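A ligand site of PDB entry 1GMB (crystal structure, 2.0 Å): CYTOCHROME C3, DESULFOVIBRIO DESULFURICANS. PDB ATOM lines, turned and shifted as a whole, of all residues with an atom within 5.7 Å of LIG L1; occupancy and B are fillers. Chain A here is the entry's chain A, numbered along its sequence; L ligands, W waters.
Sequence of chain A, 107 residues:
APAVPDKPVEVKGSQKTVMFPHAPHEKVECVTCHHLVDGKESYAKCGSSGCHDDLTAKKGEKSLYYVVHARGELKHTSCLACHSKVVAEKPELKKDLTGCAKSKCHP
Water W3 lies within hydrogen-bond range of N of Lys 12 (2.9 Å), O4 of LIG L1 (3.2 Å) and O of Glu 10 (3.3 Å).
The backbone NH of Phe 20 sits at hydrogen-bond distance from the backbone carbonyl oxygen of Val 9 (2.7 Å). OG1 of Thr 32 sits close to O of Glu 29 (3.4 Å).
Residues that only touch LIG L1: Pro 2 (3.4 Å), Ala 3 (3.7 Å), Val 4 (3.8 Å), Pro 5 (3.4 Å), Val 9 (3.8 Å), Phe 20 (3.4 Å), His 25 (3.4 Å), Val 28 (3.7 Å), Glu 29 (3.8 Å), Tyr 43 (3.5 Å) and Lys 45 (3.3 Å). 17 residues have an atom within 4 Å of LIG L1: Pro 2, Ala 3, Val 4, Pro 5, Val 9, Glu 10, Phe 20, His 22, His 25, Val 28, Glu 29, Cys 30, Cys 33, His 34, Tyr 43, Lys 45 and Cys 46. Along chain A the residues within 4 Å of LIG L1 span positions 2 to 46. The nearest printed residue that does not touch LIG L1 is Val 11 (4.04 Å).
The side-chain sulfur (SG) of Cys 33 is bonded to a carbon (C25) of LIG L1, at 1.8 Å. SG of Cys 30 is covalently linked to C18 of LIG L1 (1.8 Å). A ring nitrogen (NE2) of His 34 is bound to an iron atom (FE1) of LIG L1, 2.0 Å away. NE2 of His 22 binds FE1 of LIG L1, 2.0 Å away. The backbone carbonyl oxygen (O) of Glu 10 lies close to an oxygen (O4) of LIG L1 (2.9 Å). An oxygen (O3) of LIG L1 lies within hydrogen-bond range of the backbone NH of Cys 46, at 3.3 Å. A ring nitrogen (NE2) of His 25 binds an iron atom (FE1) of LG2 L2, at 2.0 Å. The side-chain sulfur (SG) of Cys 46 is covalently linked to a carbon (C18) of LG3 L3 (1.8 Å).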
ATOM      1  N   ALA A   1      -4.840   0.308  -6.684  1.00  0.00           N
ATOM      2  CA  ALA A   1      -5.685   0.662  -7.869  1.00  0.00           C
ATOM      3  C   ALA A   1      -5.116   1.987  -8.385  1.00  0.00           C
ATOM      4  O   ALA A   1      -4.224   2.559  -7.750  1.00  0.00           O
ATOM      5  CB  ALA A   1      -7.126   0.833  -7.417  1.00  0.00           C
ATOM      6  N   PRO A   2      -5.579   2.469  -9.563  1.00  0.00           N
ATOM      7  CA  PRO A   2      -5.022   3.744 -10.031  1.00  0.00           C
ATOM      8  C   PRO A   2      -5.348   4.856  -9.038  1.00  0.00           C
ATOM      9  O   PRO A   2      -6.187   4.677  -8.136  1.00  0.00           O
ATOM     10  CB  PRO A   2      -5.761   3.982 -11.352  1.00  0.00           C
ATOM     11  CG  PRO A   2      -7.064   3.264 -11.165  1.00  0.00           C
ATOM     12  CD  PRO A   2      -6.602   1.982 -10.500  1.00  0.00           C
ATOM     13  N   ALA A   3      -4.650   5.973  -9.144  1.00  0.00           N
ATOM     14  CA  ALA A   3      -4.957   7.068  -8.237  1.00  0.00           C
ATOM     15  C   ALA A   3      -6.333   7.633  -8.653  1.00  0.00           C
ATOM     16  O   ALA A   3      -6.677   7.706  -9.841  1.00  0.00           O
ATOM     17  CB  ALA A   3      -3.881   8.152  -8.326  1.00  0.00           C
ATOM     18  N   VAL A   4      -7.145   7.984  -7.661  1.00  0.00           N
ATOM     19  CA  VAL A   4      -8.459   8.551  -7.938  1.00  0.00           C
ATOM     20  C   VAL A   4      -8.231   9.963  -8.554  1.00  0.00           C
ATOM     21  O   VAL A   4      -7.280  10.654  -8.178  1.00  0.00           O
ATOM     22  CB  VAL A   4      -9.254   8.602  -6.608  1.00  0.00           C
ATOM     23  CG1 VAL A   4      -8.625   9.569  -5.635  1.00  0.00           C
ATOM     24  CG2 VAL A   4     -10.684   8.924  -6.852  1.00  0.00           C
ATOM     25  N   PRO A   5      -9.014  10.359  -9.585  1.00  0.00           N
ATOM     26  CA  PRO A   5      -8.839  11.683 -10.218  1.00  0.00           C
ATOM     27  C   PRO A   5      -8.995  12.814  -9.191  1.00  0.00           C
ATOM     28  O   PRO A   5      -9.907  12.780  -8.364  1.00  0.00           O
ATOM     29  CB  PRO A   5      -9.973  11.723 -11.247  1.00  0.00           C
ATOM     30  CG  PRO A   5     -10.096  10.311 -11.651  1.00  0.00           C
ATOM     31  CD  PRO A   5     -10.024   9.570 -10.315  1.00  0.00           C
ATOM     32  N   VAL A   9     -14.174  15.071 -13.460  1.00  0.00           N
ATOM     33  CA  VAL A   9     -14.029  14.394 -14.740  1.00  0.00           C
ATOM     34  C   VAL A   9     -15.334  14.380 -15.519  1.00  0.00           C
ATOM     35  O   VAL A   9     -16.418  14.387 -14.932  1.00  0.00           O
ATOM     36  CB  VAL A   9     -13.542  12.921 -14.576  1.00  0.00           C
ATOM     37  CG1 VAL A   9     -12.115  12.891 -14.072  1.00  0.00           C
ATOM     38  CG2 VAL A   9     -14.477  12.152 -13.644  1.00  0.00           C
ATOM     39  N   GLU A  10     -15.227  14.173 -16.755  1.00  0.00           N
ATOM     40  CA  GLU A  10     -16.373  14.256 -17.657  1.00  0.00           C
ATOM     41  C   GLU A  10     -17.107  12.928 -17.781  1.00  0.00           C
ATOM     42  O   GLU A  10     -16.491  11.883 -18.031  1.00  0.00           O
ATOM     43  CB  GLU A  10     -15.953  14.619 -19.084  1.00  0.00           C
ATOM     44  CG  GLU A  10     -15.678  16.098 -19.314  1.00  0.00           C
ATOM     45  CD  GLU A  10     -15.561  16.448 -20.794  1.00  0.00           C
ATOM     46  OE1 GLU A  10     -14.687  15.852 -21.536  1.00  0.00           O
ATOM     47  OE2 GLU A  10     -16.341  17.331 -21.322  1.00  0.00           O
ATOM     48  N   VAL A  11     -18.394  13.019 -17.598  1.00  0.00           N
ATOM     49  CA  VAL A  11     -19.302  11.896 -17.776  1.00  0.00           C
ATOM     50  C   VAL A  11     -20.158  12.282 -18.974  1.00  0.00           C
ATOM     51  O   VAL A  11     -21.146  13.004 -18.842  1.00  0.00           O
ATOM     52  CB  VAL A  11     -20.167  11.655 -16.529  1.00  0.00           C
ATOM     53  CG1 VAL A  11     -21.058  10.414 -16.655  1.00  0.00           C
ATOM     54  CG2 VAL A  11     -19.353  11.457 -15.258  1.00  0.00           C
ATOM     55  N   LYS A  12     -19.730  11.805 -20.116  1.00  0.00           N
ATOM     56  CA  LYS A  12     -20.390  12.099 -21.391  1.00  0.00           C
ATOM     57  C   LYS A  12     -21.603  11.191 -21.596  1.00  0.00           C
ATOM     58  O   LYS A  12     -21.472   9.984 -21.850  1.00  0.00           O
ATOM     59  CB  LYS A  12     -19.409  11.890 -22.541  1.00  0.00           C
ATOM     60  CG  LYS A  12     -18.266  12.917 -22.548  1.00  0.00           C
ATOM     61  CD  LYS A  12     -17.347  12.764 -23.757  1.00  0.00           C
ATOM     62  CE  LYS A  12     -16.282  13.856 -23.860  1.00  0.00           C
ATOM     63  NZ  LYS A  12     -15.537  13.818 -25.125  1.00  0.00           N
ATOM     64  N   PHE A  20     -18.135  14.871 -12.917  1.00  0.00           N
ATOM     65  CA  PHE A  20     -18.165  14.084 -11.689  1.00  0.00           C
ATOM     66  C   PHE A  20     -16.989  14.425 -10.801  1.00  0.00           C
ATOM     67  O   PHE A  20     -15.832  14.281 -11.220  1.00  0.00           O
ATOM     68  CB  PHE A  20     -18.129  12.584 -11.977  1.00  0.00           C
ATOM     69  CG  PHE A  20     -18.086  11.746 -10.740  1.00  0.00           C
ATOM     70  CD1 PHE A  20     -19.228  11.586  -9.970  1.00  0.00           C
ATOM     71  CD2 PHE A  20     -16.893  11.197 -10.295  1.00  0.00           C
ATOM     72  CE1 PHE A  20     -19.188  10.887  -8.768  1.00  0.00           C
ATOM     73  CE2 PHE A  20     -16.847  10.494  -9.086  1.00  0.00           C
ATOM     74  CZ  PHE A  20     -18.000  10.344  -8.330  1.00  0.00           C
ATOM     75  N   HIS A  22     -14.752  13.527  -7.548  1.00  0.00           N
ATOM     76  CA  HIS A  22     -14.426  12.442  -6.609  1.00  0.00           C
ATOM     77  C   HIS A  22     -14.301  12.844  -5.126  1.00  0.00           C
ATOM     78  O   HIS A  22     -14.708  12.098  -4.246  1.00  0.00           O
ATOM     79  CB  HIS A  22     -13.140  11.728  -7.040  1.00  0.00           C
ATOM     80  CG  HIS A  22     -13.343  10.683  -8.093  1.00  0.00           C
ATOM     81  ND1 HIS A  22     -13.258  10.912  -9.438  1.00  0.00           N
ATOM     82  CD2 HIS A  22     -13.564   9.348  -7.956  1.00  0.00           C
ATOM     83  CE1 HIS A  22     -13.405   9.750 -10.077  1.00  0.00           C
ATOM     84  NE2 HIS A  22     -13.604   8.764  -9.225  1.00  0.00           N
ATOM     85  N   HIS A  25     -16.862  12.168  -2.519  1.00  0.00           N
ATOM     86  CA  HIS A  25     -17.139  10.735  -2.403  1.00  0.00           C
ATOM     87  C   HIS A  25     -15.934   9.997  -1.832  1.00  0.00           C
ATOM     88  O   HIS A  25     -15.849   8.780  -1.938  1.00  0.00           O
ATOM     89  CB  HIS A  25     -17.489  10.153  -3.781  1.00  0.00           C
ATOM     90  CG  HIS A  25     -18.639  10.824  -4.457  1.00  0.00           C
ATOM     91  ND1 HIS A  25     -18.502  11.936  -5.260  1.00  0.00           N
ATOM     92  CD2 HIS A  25     -19.962  10.564  -4.409  1.00  0.00           C
ATOM     93  CE1 HIS A  25     -19.724  12.301  -5.675  1.00  0.00           C
ATOM     94  NE2 HIS A  25     -20.647  11.502  -5.183  1.00  0.00           N
ATOM     95  N   VAL A  28     -16.776   6.979   0.097  1.00  0.00           N
ATOM     96  CA  VAL A  28     -17.488   5.894  -0.567  1.00  0.00           C
ATOM     97  C   VAL A  28     -16.427   4.948  -1.159  1.00  0.00           C
ATOM     98  O   VAL A  28     -15.468   5.391  -1.776  1.00  0.00           O
ATOM     99  CB  VAL A  28     -18.397   6.410  -1.706  1.00  0.00           C
ATOM    100  CG1 VAL A  28     -19.171   5.262  -2.303  1.00  0.00           C
ATOM    101  CG2 VAL A  28     -19.346   7.493  -1.215  1.00  0.00           C
ATOM    102  N   GLU A  29     -16.619   3.634  -0.987  1.00  0.00           N
ATOM    103  CA  GLU A  29     -15.688   2.645  -1.531  1.00  0.00           C
ATOM    104  C   GLU A  29     -15.692   2.712  -3.045  1.00  0.00           C
ATOM    105  O   GLU A  29     -16.753   2.768  -3.671  1.00  0.00           O
ATOM    106  CB  GLU A  29     -16.112   1.230  -1.136  1.00  0.00           C
ATOM    107  CG  GLU A  29     -16.020   0.938   0.329  1.00  0.00           C
ATOM    108  CD  GLU A  29     -16.453  -0.467   0.680  1.00  0.00           C
ATOM    109  OE1 GLU A  29     -17.110  -1.136  -0.141  1.00  0.00           O
ATOM    110  OE2 GLU A  29     -16.122  -0.902   1.793  1.00  0.00           O
ATOM    111  N   CYS A  30     -14.514   2.609  -3.643  1.00  0.00           N
ATOM    112  CA  CYS A  30     -14.379   2.650  -5.099  1.00  0.00           C
ATOM    113  C   CYS A  30     -15.328   1.677  -5.784  1.00  0.00           C
ATOM    114  O   CYS A  30     -15.974   2.021  -6.774  1.00  0.00           O
ATOM    115  CB  CYS A  30     -12.958   2.296  -5.526  1.00  0.00           C
ATOM    116  SG  CYS A  30     -11.673   3.236  -4.731  1.00  0.00           S
ATOM    117  N   THR A  32     -18.187   0.629  -5.012  1.00  0.00           N
ATOM    118  CA  THR A  32     -19.595   0.993  -5.041  1.00  0.00           C
ATOM    119  C   THR A  32     -19.964   1.485  -6.435  1.00  0.00           C
ATOM    120  O   THR A  32     -21.010   1.124  -6.961  1.00  0.00           O
ATOM    121  CB  THR A  32     -19.914   2.087  -4.008  1.00  0.00           C
ATOM    122  OG1 THR A  32     -19.751   1.537  -2.690  1.00  0.00           O
ATOM    123  CG2 THR A  32     -21.358   2.614  -4.160  1.00  0.00           C
ATOM    124  N   CYS A  33     -19.095   2.291  -7.039  1.00  0.00           N
ATOM    125  CA  CYS A  33     -19.340   2.821  -8.378  1.00  0.00           C
ATOM    126  C   CYS A  33     -18.586   2.001  -9.420  1.00  0.00           C
ATOM    127  O   CYS A  33     -19.164   1.580 -10.416  1.00  0.00           O
ATOM    128  CB  CYS A  33     -18.933   4.286  -8.432  1.00  0.00           C
ATOM    129  SG  CYS A  33     -19.777   5.252  -7.201  1.00  0.00           S
ATOM    130  N   HIS A  34     -17.291   1.803  -9.201  1.00  0.00           N
ATOM    131  CA  HIS A  34     -16.479   0.994 -10.094  1.00  0.00           C
ATOM    132  C   HIS A  34     -16.653  -0.453  -9.633  1.00  0.00           C
ATOM    133  O   HIS A  34     -15.745  -1.074  -9.077  1.00  0.00           O
ATOM    134  CB  HIS A  34     -15.007   1.407 -10.028  1.00  0.00           C
ATOM    135  CG  HIS A  34     -14.787   2.847 -10.371  1.00  0.00           C
ATOM    136  ND1 HIS A  34     -14.880   3.347 -11.650  1.00  0.00           N
ATOM    137  CD2 HIS A  34     -14.532   3.907  -9.568  1.00  0.00           C
ATOM    138  CE1 HIS A  34     -14.692   4.671 -11.591  1.00  0.00           C
ATOM    139  NE2 HIS A  34     -14.479   5.061 -10.348  1.00  0.00           N
ATOM    140  N   TYR A  43     -11.855   0.003 -13.580  1.00  0.00           N
ATOM    141  CA  TYR A  43     -12.015   1.422 -13.378  1.00  0.00           C
ATOM    142  C   TYR A  43     -12.259   2.081 -14.732  1.00  0.00           C
ATOM    143  O   TYR A  43     -12.076   3.283 -14.898  1.00  0.00           O
ATOM    144  CB  TYR A  43     -10.737   1.983 -12.730  1.00  0.00           C
ATOM    145  CG  TYR A  43     -10.544   1.508 -11.313  1.00  0.00           C
ATOM    146  CD1 TYR A  43      -9.788   0.360 -11.032  1.00  0.00           C
ATOM    147  CD2 TYR A  43     -11.158   2.172 -10.256  1.00  0.00           C
ATOM    148  CE1 TYR A  43      -9.661  -0.100  -9.710  1.00  0.00           C
ATOM    149  CE2 TYR A  43     -11.031   1.730  -8.951  1.00  0.00           C
ATOM    150  CZ  TYR A  43     -10.294   0.592  -8.677  1.00  0.00           C
ATOM    151  OH  TYR A  43     -10.205   0.151  -7.371  1.00  0.00           O
ATOM    152  N   ALA A  44     -12.686   1.281 -15.698  1.00  0.00           N
ATOM    153  CA  ALA A  44     -12.943   1.775 -17.051  1.00  0.00           C
ATOM    154  C   ALA A  44     -14.138   2.729 -17.015  1.00  0.00           C
ATOM    155  O   ALA A  44     -14.941   2.674 -16.087  1.00  0.00           O
ATOM    156  CB  ALA A  44     -13.217   0.605 -17.985  1.00  0.00           C
ATOM    157  N   LYS A  45     -14.252   3.579 -18.024  1.00  0.00           N
ATOM    158  CA  LYS A  45     -15.365   4.520 -18.109  1.00  0.00           C
ATOM    159  C   LYS A  45     -16.690   3.782 -18.136  1.00  0.00           C
ATOM    160  O   LYS A  45     -16.828   2.768 -18.813  1.00  0.00           O
ATOM    161  CB  LYS A  45     -15.220   5.400 -19.355  1.00  0.00           C
ATOM    162  CG  LYS A  45     -14.136   6.445 -19.213  1.00  0.00           C
ATOM    163  CD  LYS A  45     -13.934   7.270 -20.484  1.00  0.00           C
ATOM    164  CE  LYS A  45     -12.996   8.445 -20.207  1.00  0.00           C
ATOM    165  NZ  LYS A  45     -12.080   8.671 -21.346  1.00  0.00           N
ATOM    166  N   CYS A  46     -17.670   4.291 -17.396  1.00  0.00           N
ATOM    167  CA  CYS A  46     -18.973   3.642 -17.352  1.00  0.00           C
ATOM    168  C   CYS A  46     -19.560   3.390 -18.736  1.00  0.00           C
ATOM    169  O   CYS A  46     -20.083   2.306 -18.998  1.00  0.00           O
ATOM    170  CB  CYS A  46     -19.958   4.486 -16.541  1.00  0.00           C
ATOM    171  SG  CYS A  46     -19.293   5.083 -14.987  1.00  0.00           S
ATOM    172  N   GLY A  47     -19.443   4.374 -19.625  1.00  0.00           N
ATOM    173  CA  GLY A  47     -19.978   4.228 -20.979  1.00  0.00           C
ATOM    174  C   GLY A  47     -19.070   3.531 -21.977  1.00  0.00           C
ATOM    175  O   GLY A  47     -19.207   3.722 -23.182  1.00  0.00           O
ATOM    176  N   LEU A  64     -26.607   4.141 -20.070  1.00  0.00           N
ATOM    177  CA  LEU A  64     -25.811   4.918 -19.129  1.00  0.00           C
ATOM    178  C   LEU A  64     -26.767   5.801 -18.330  1.00  0.00           C
ATOM    179  O   LEU A  64     -26.613   5.977 -17.125  1.00  0.00           O
ATOM    180  CB  LEU A  64     -24.777   5.777 -19.863  1.00  0.00           C
ATOM    181  CG  LEU A  64     -23.813   6.600 -18.984  1.00  0.00           C
ATOM    182  CD1 LEU A  64     -23.085   5.678 -18.031  1.00  0.00           C
ATOM    183  CD2 LEU A  64     -22.826   7.354 -19.838  1.00  0.00           C
HETATM  184 FE1  LIG L   1     -13.990   6.907  -9.818  1.00  0.00          FE
HETATM  185  C1  LIG L   1     -13.696   7.945 -12.991  1.00  0.00           C
HETATM  186  C2  LIG L   1     -10.757   5.908  -9.773  1.00  0.00           C
HETATM  187  C3  LIG L   1     -14.264   6.056  -6.592  1.00  0.00           C
HETATM  188  C4  LIG L   1     -17.344   7.221 -10.052  1.00  0.00           C
HETATM  189  N1  LIG L   1     -12.543   6.924 -11.081  1.00  0.00           N
HETATM  190  C5  LIG L   1     -12.564   7.391 -12.368  1.00  0.00           C
HETATM  191  C6  LIG L   1     -11.250   7.183 -12.958  1.00  0.00           C
HETATM  192  C7  LIG L   1     -10.449   6.587 -12.092  1.00  0.00           C
HETATM  193  C8  LIG L   1     -11.255   6.444 -10.915  1.00  0.00           C
HETATM  194  C9  LIG L   1      -8.979   6.199 -12.334  1.00  0.00           C
HETATM  195  C10 LIG L   1     -10.837   7.639 -14.331  1.00  0.00           C
HETATM  196  C11 LIG L   1     -11.336   6.689 -15.399  1.00  0.00           C
HETATM  197  C12 LIG L   1     -11.834   7.432 -16.605  1.00  0.00           C
HETATM  198  O1  LIG L   1     -12.976   7.942 -16.549  1.00  0.00           O
HETATM  199  O2  LIG L   1     -11.087   7.511 -17.602  1.00  0.00           O
HETATM  200  N2  LIG L   1     -12.752   6.110  -8.452  1.00  0.00           N
HETATM  201  C13 LIG L   1     -11.456   5.706  -8.622  1.00  0.00           C
HETATM  202  C14 LIG L   1     -10.874   5.163  -7.393  1.00  0.00           C
HETATM  203  C15 LIG L   1     -11.857   5.280  -6.434  1.00  0.00           C
HETATM  204  C16 LIG L   1     -13.034   5.849  -7.142  1.00  0.00           C
HETATM  205  C17 LIG L   1      -9.479   4.561  -7.237  1.00  0.00           C
HETATM  206  C18 LIG L   1     -11.769   5.035  -5.052  1.00  0.00           C
HETATM  207  C19 LIG L   1     -10.796   5.693  -4.162  1.00  0.00           C
HETATM  208  N3  LIG L   1     -15.490   6.695  -8.586  1.00  0.00           N
HETATM  209  C20 LIG L   1     -15.415   6.427  -7.251  1.00  0.00           C
HETATM  210  C21 LIG L   1     -16.720   6.514  -6.618  1.00  0.00           C
HETATM  211  C22 LIG L   1     -17.627   6.822  -7.579  1.00  0.00           C
HETATM  212  C23 LIG L   1     -16.831   6.890  -8.814  1.00  0.00           C
HETATM  213  C24 LIG L   1     -17.017   6.269  -5.138  1.00  0.00           C
HETATM  214  C25 LIG L   1     -19.036   6.906  -7.417  1.00  0.00           C
HETATM  215  C26 LIG L   1     -19.653   7.845  -6.508  1.00  0.00           C
HETATM  216  N4  LIG L   1     -15.253   7.521 -11.213  1.00  0.00           N
HETATM  217  C27 LIG L   1     -16.631   7.557 -11.154  1.00  0.00           C
HETATM  218  C28 LIG L   1     -17.211   8.127 -12.365  1.00  0.00           C
HETATM  219  C29 LIG L   1     -16.161   8.405 -13.185  1.00  0.00           C
HETATM  220  C30 LIG L   1     -14.962   8.005 -12.467  1.00  0.00           C
HETATM  221  C31 LIG L   1     -18.682   8.436 -12.658  1.00  0.00           C
HETATM  222  C32 LIG L   1     -16.268   8.933 -14.608  1.00  0.00           C
HETATM  223  C33 LIG L   1     -16.263   7.763 -15.581  1.00  0.00           C
HETATM  224  C34 LIG L   1     -16.768   8.149 -16.935  1.00  0.00           C
HETATM  225  O3  LIG L   1     -17.784   7.585 -17.375  1.00  0.00           O
HETATM  226  O4  LIG L   1     -16.161   9.041 -17.558  1.00  0.00           O
HETATM  227 FE1  LG2 L   2     -22.556  11.910  -5.239  1.00  0.00          FE
HETATM  228  C1  LG2 L   2     -22.084  14.822  -3.577  1.00  0.00           C
HETATM  229  C2  LG2 L   2     -22.339  13.538  -8.242  1.00  0.00           C
HETATM  230  C3  LG2 L   2     -22.942   8.943  -6.921  1.00  0.00           C
HETATM  231  C4  LG2 L   2     -22.939  10.236  -2.263  1.00  0.00           C
HETATM  232  N1  LG2 L   2     -22.312  13.737  -5.776  1.00  0.00           N
HETATM  233  C5  LG2 L   2     -22.157  14.834  -4.954  1.00  0.00           C
HETATM  234  C6  LG2 L   2     -22.133  16.015  -5.721  1.00  0.00           C
HETATM  235  C7  LG2 L   2     -22.188  15.704  -7.041  1.00  0.00           C
HETATM  236  C8  LG2 L   2     -22.280  14.270  -7.077  1.00  0.00           C
HETATM  237  C9  LG2 L   2     -22.193  16.675  -8.219  1.00  0.00           C
HETATM  238  C10 LG2 L   2     -22.165  17.409  -5.144  1.00  0.00           C
HETATM  239  C11 LG2 L   2     -20.801  17.986  -4.863  1.00  0.00           C
HETATM  240  C12 LG2 L   2     -20.860  19.493  -4.712  1.00  0.00           C
HETATM  241  O1  LG2 L   2     -21.107  19.972  -3.586  1.00  0.00           O
HETATM  242  O2  LG2 L   2     -20.691  20.186  -5.739  1.00  0.00           O
HETATM  243  N2  LG2 L   2     -22.629  11.374  -7.192  1.00  0.00           N
HETATM  244  C13 LG2 L   2     -22.554  12.178  -8.302  1.00  0.00           C
HETATM  245  C14 LG2 L   2     -22.714  11.407  -9.511  1.00  0.00           C
HETATM  246  C15 LG2 L   2     -22.803  10.107  -9.151  1.00  0.00           C
HETATM  247  C16 LG2 L   2     -22.794  10.090  -7.710  1.00  0.00           C
HETATM  248  C17 LG2 L   2     -22.908  11.990 -10.913  1.00  0.00           C
HETATM  249  C18 LG2 L   2     -22.848   8.999 -10.012  1.00  0.00           C
HETATM  250  C19 LG2 L   2     -21.757   8.701 -10.919  1.00  0.00           C
HETATM  251  N3  LG2 L   2     -22.894   9.990  -4.672  1.00  0.00           N
HETATM  252  C20 LG2 L   2     -22.997   8.888  -5.526  1.00  0.00           C
HETATM  253  C21 LG2 L   2     -23.149   7.661  -4.788  1.00  0.00           C
HETATM  254  C22 LG2 L   2     -23.183   8.040  -3.450  1.00  0.00           C
HETATM  255  C23 LG2 L   2     -23.032   9.473  -3.406  1.00  0.00           C
HETATM  256  C24 LG2 L   2     -23.260   6.279  -5.444  1.00  0.00           C
HETATM  257  C25 LG2 L   2     -23.407   7.270  -2.300  1.00  0.00           C
HETATM  258  C26 LG2 L   2     -22.880   5.908  -2.137  1.00  0.00           C
HETATM  259  N4  LG2 L   2     -22.524  12.407  -3.350  1.00  0.00           N
HETATM  260  C27 LG2 L   2     -22.635  11.591  -2.236  1.00  0.00           C
HETATM  261  C28 LG2 L   2     -22.327  12.332  -1.021  1.00  0.00           C
HETATM  262  C29 LG2 L   2     -22.130  13.639  -1.406  1.00  0.00           C
HETATM  263  C30 LG2 L   2     -22.242  13.684  -2.832  1.00  0.00           C
HETATM  264  C31 LG2 L   2     -22.146  11.736   0.397  1.00  0.00           C
HETATM  265  C32 LG2 L   2     -21.870  14.828  -0.506  1.00  0.00           C
HETATM  266  C33 LG2 L   2     -23.107  15.354   0.238  1.00  0.00           C
HETATM  267  C34 LG2 L   2     -22.759  16.288   1.390  1.00  0.00           C
HETATM  268  O3  LG2 L   2     -22.247  17.418   1.152  1.00  0.00           O
HETATM  269  O4  LG2 L   2     -23.024  15.890   2.549  1.00  0.00           O
HETATM  270 FE1  LG3 L   3     -21.881  -1.109 -14.627  1.00  0.00          FE
HETATM  271  C1  LG3 L   3     -24.464  -3.149 -13.921  1.00  0.00           C
HETATM  272  C2  LG3 L   3     -23.216   1.398 -12.795  1.00  0.00           C
HETATM  273  C3  LG3 L   3     -19.001   0.766 -14.972  1.00  0.00           C
HETATM  274  C4  LG3 L   3     -20.639  -3.448 -16.824  1.00  0.00           C
HETATM  275  N1  LG3 L   3     -23.513  -0.928 -13.589  1.00  0.00           N
HETATM  276  C5  LG3 L   3     -24.478  -1.876 -13.368  1.00  0.00           C
HETATM  277  C6  LG3 L   3     -25.556  -1.343 -12.574  1.00  0.00           C
HETATM  278  C7  LG3 L   3     -25.212  -0.082 -12.293  1.00  0.00           C
HETATM  279  C8  LG3 L   3     -23.954   0.186 -12.924  1.00  0.00           C
HETATM  280  C9  LG3 L   3     -25.951   0.873 -11.375  1.00  0.00           C
HETATM  281  C10 LG3 L   3     -26.848  -2.055 -12.216  1.00  0.00           C
HETATM  282  C11 LG3 L   3     -27.738  -2.003 -13.452  1.00  0.00           C
HETATM  283  C12 LG3 L   3     -28.996  -2.856 -13.335  1.00  0.00           C
HETATM  284  O1  LG3 L   3     -29.249  -3.441 -12.254  1.00  0.00           O
HETATM  285  O2  LG3 L   3     -29.722  -2.953 -14.339  1.00  0.00           O
HETATM  286  N2  LG3 L   3     -21.222   0.756 -14.033  1.00  0.00           N
HETATM  287  C13 LG3 L   3     -21.952   1.673 -13.308  1.00  0.00           C
HETATM  288  C14 LG3 L   3     -21.234   2.916 -13.156  1.00  0.00           C
HETATM  289  C15 LG3 L   3     -20.010   2.732 -13.730  1.00  0.00           C
HETATM  290  C16 LG3 L   3     -20.018   1.360 -14.245  1.00  0.00           C
HETATM  291  C17 LG3 L   3     -21.791   4.207 -12.554  1.00  0.00           C
HETATM  292  C18 LG3 L   3     -18.986   3.691 -13.832  1.00  0.00           C
HETATM  293  C19 LG3 L   3     -18.326   4.176 -12.613  1.00  0.00           C
HETATM  294  N3  LG3 L   3     -20.198  -1.277 -15.712  1.00  0.00           N
HETATM  295  C20 LG3 L   3     -19.078  -0.441 -15.699  1.00  0.00           C
HETATM  296  C21 LG3 L   3     -18.055  -0.931 -16.607  1.00  0.00           C
HETATM  297  C22 LG3 L   3     -18.540  -2.070 -17.216  1.00  0.00           C
HETATM  298  C23 LG3 L   3     -19.864  -2.296 -16.634  1.00  0.00           C
HETATM  299  C24 LG3 L   3     -16.702  -0.253 -16.906  1.00  0.00           C
HETATM  300  C25 LG3 L   3     -17.951  -2.766 -18.287  1.00  0.00           C
HETATM  301  C26 LG3 L   3     -16.605  -3.291 -18.113  1.00  0.00           C
HETATM  302  N4  LG3 L   3     -22.441  -2.931 -15.243  1.00  0.00           N
HETATM  303  C27 LG3 L   3     -21.805  -3.772 -16.160  1.00  0.00           C
HETATM  304  C28 LG3 L   3     -22.477  -5.070 -16.241  1.00  0.00           C
HETATM  305  C29 LG3 L   3     -23.565  -4.967 -15.440  1.00  0.00           C
HETATM  306  C30 LG3 L   3     -23.529  -3.651 -14.810  1.00  0.00           C
HETATM  307  C31 LG3 L   3     -22.027  -6.339 -17.004  1.00  0.00           C
HETATM  308  C32 LG3 L   3     -24.597  -6.054 -15.155  1.00  0.00           C
HETATM  309  C33 LG3 L   3     -24.527  -6.514 -13.700  1.00  0.00           C
HETATM  310  C34 LG3 L   3     -23.172  -7.082 -13.341  1.00  0.00           C
HETATM  311  O3  LG3 L   3     -22.673  -7.955 -14.065  1.00  0.00           O
HETATM  312  O4  LG3 L   3     -22.584  -6.652 -12.319  1.00  0.00           O
HETATM  313  O   HOH W   1      -9.857  10.074 -16.638  1.00  0.00           O
HETATM  314  O   HOH W   2     -13.604   7.149  -2.974  1.00  0.00           O
HETATM  315  O   HOH W   3     -17.622   9.826 -20.310  1.00  0.00           O
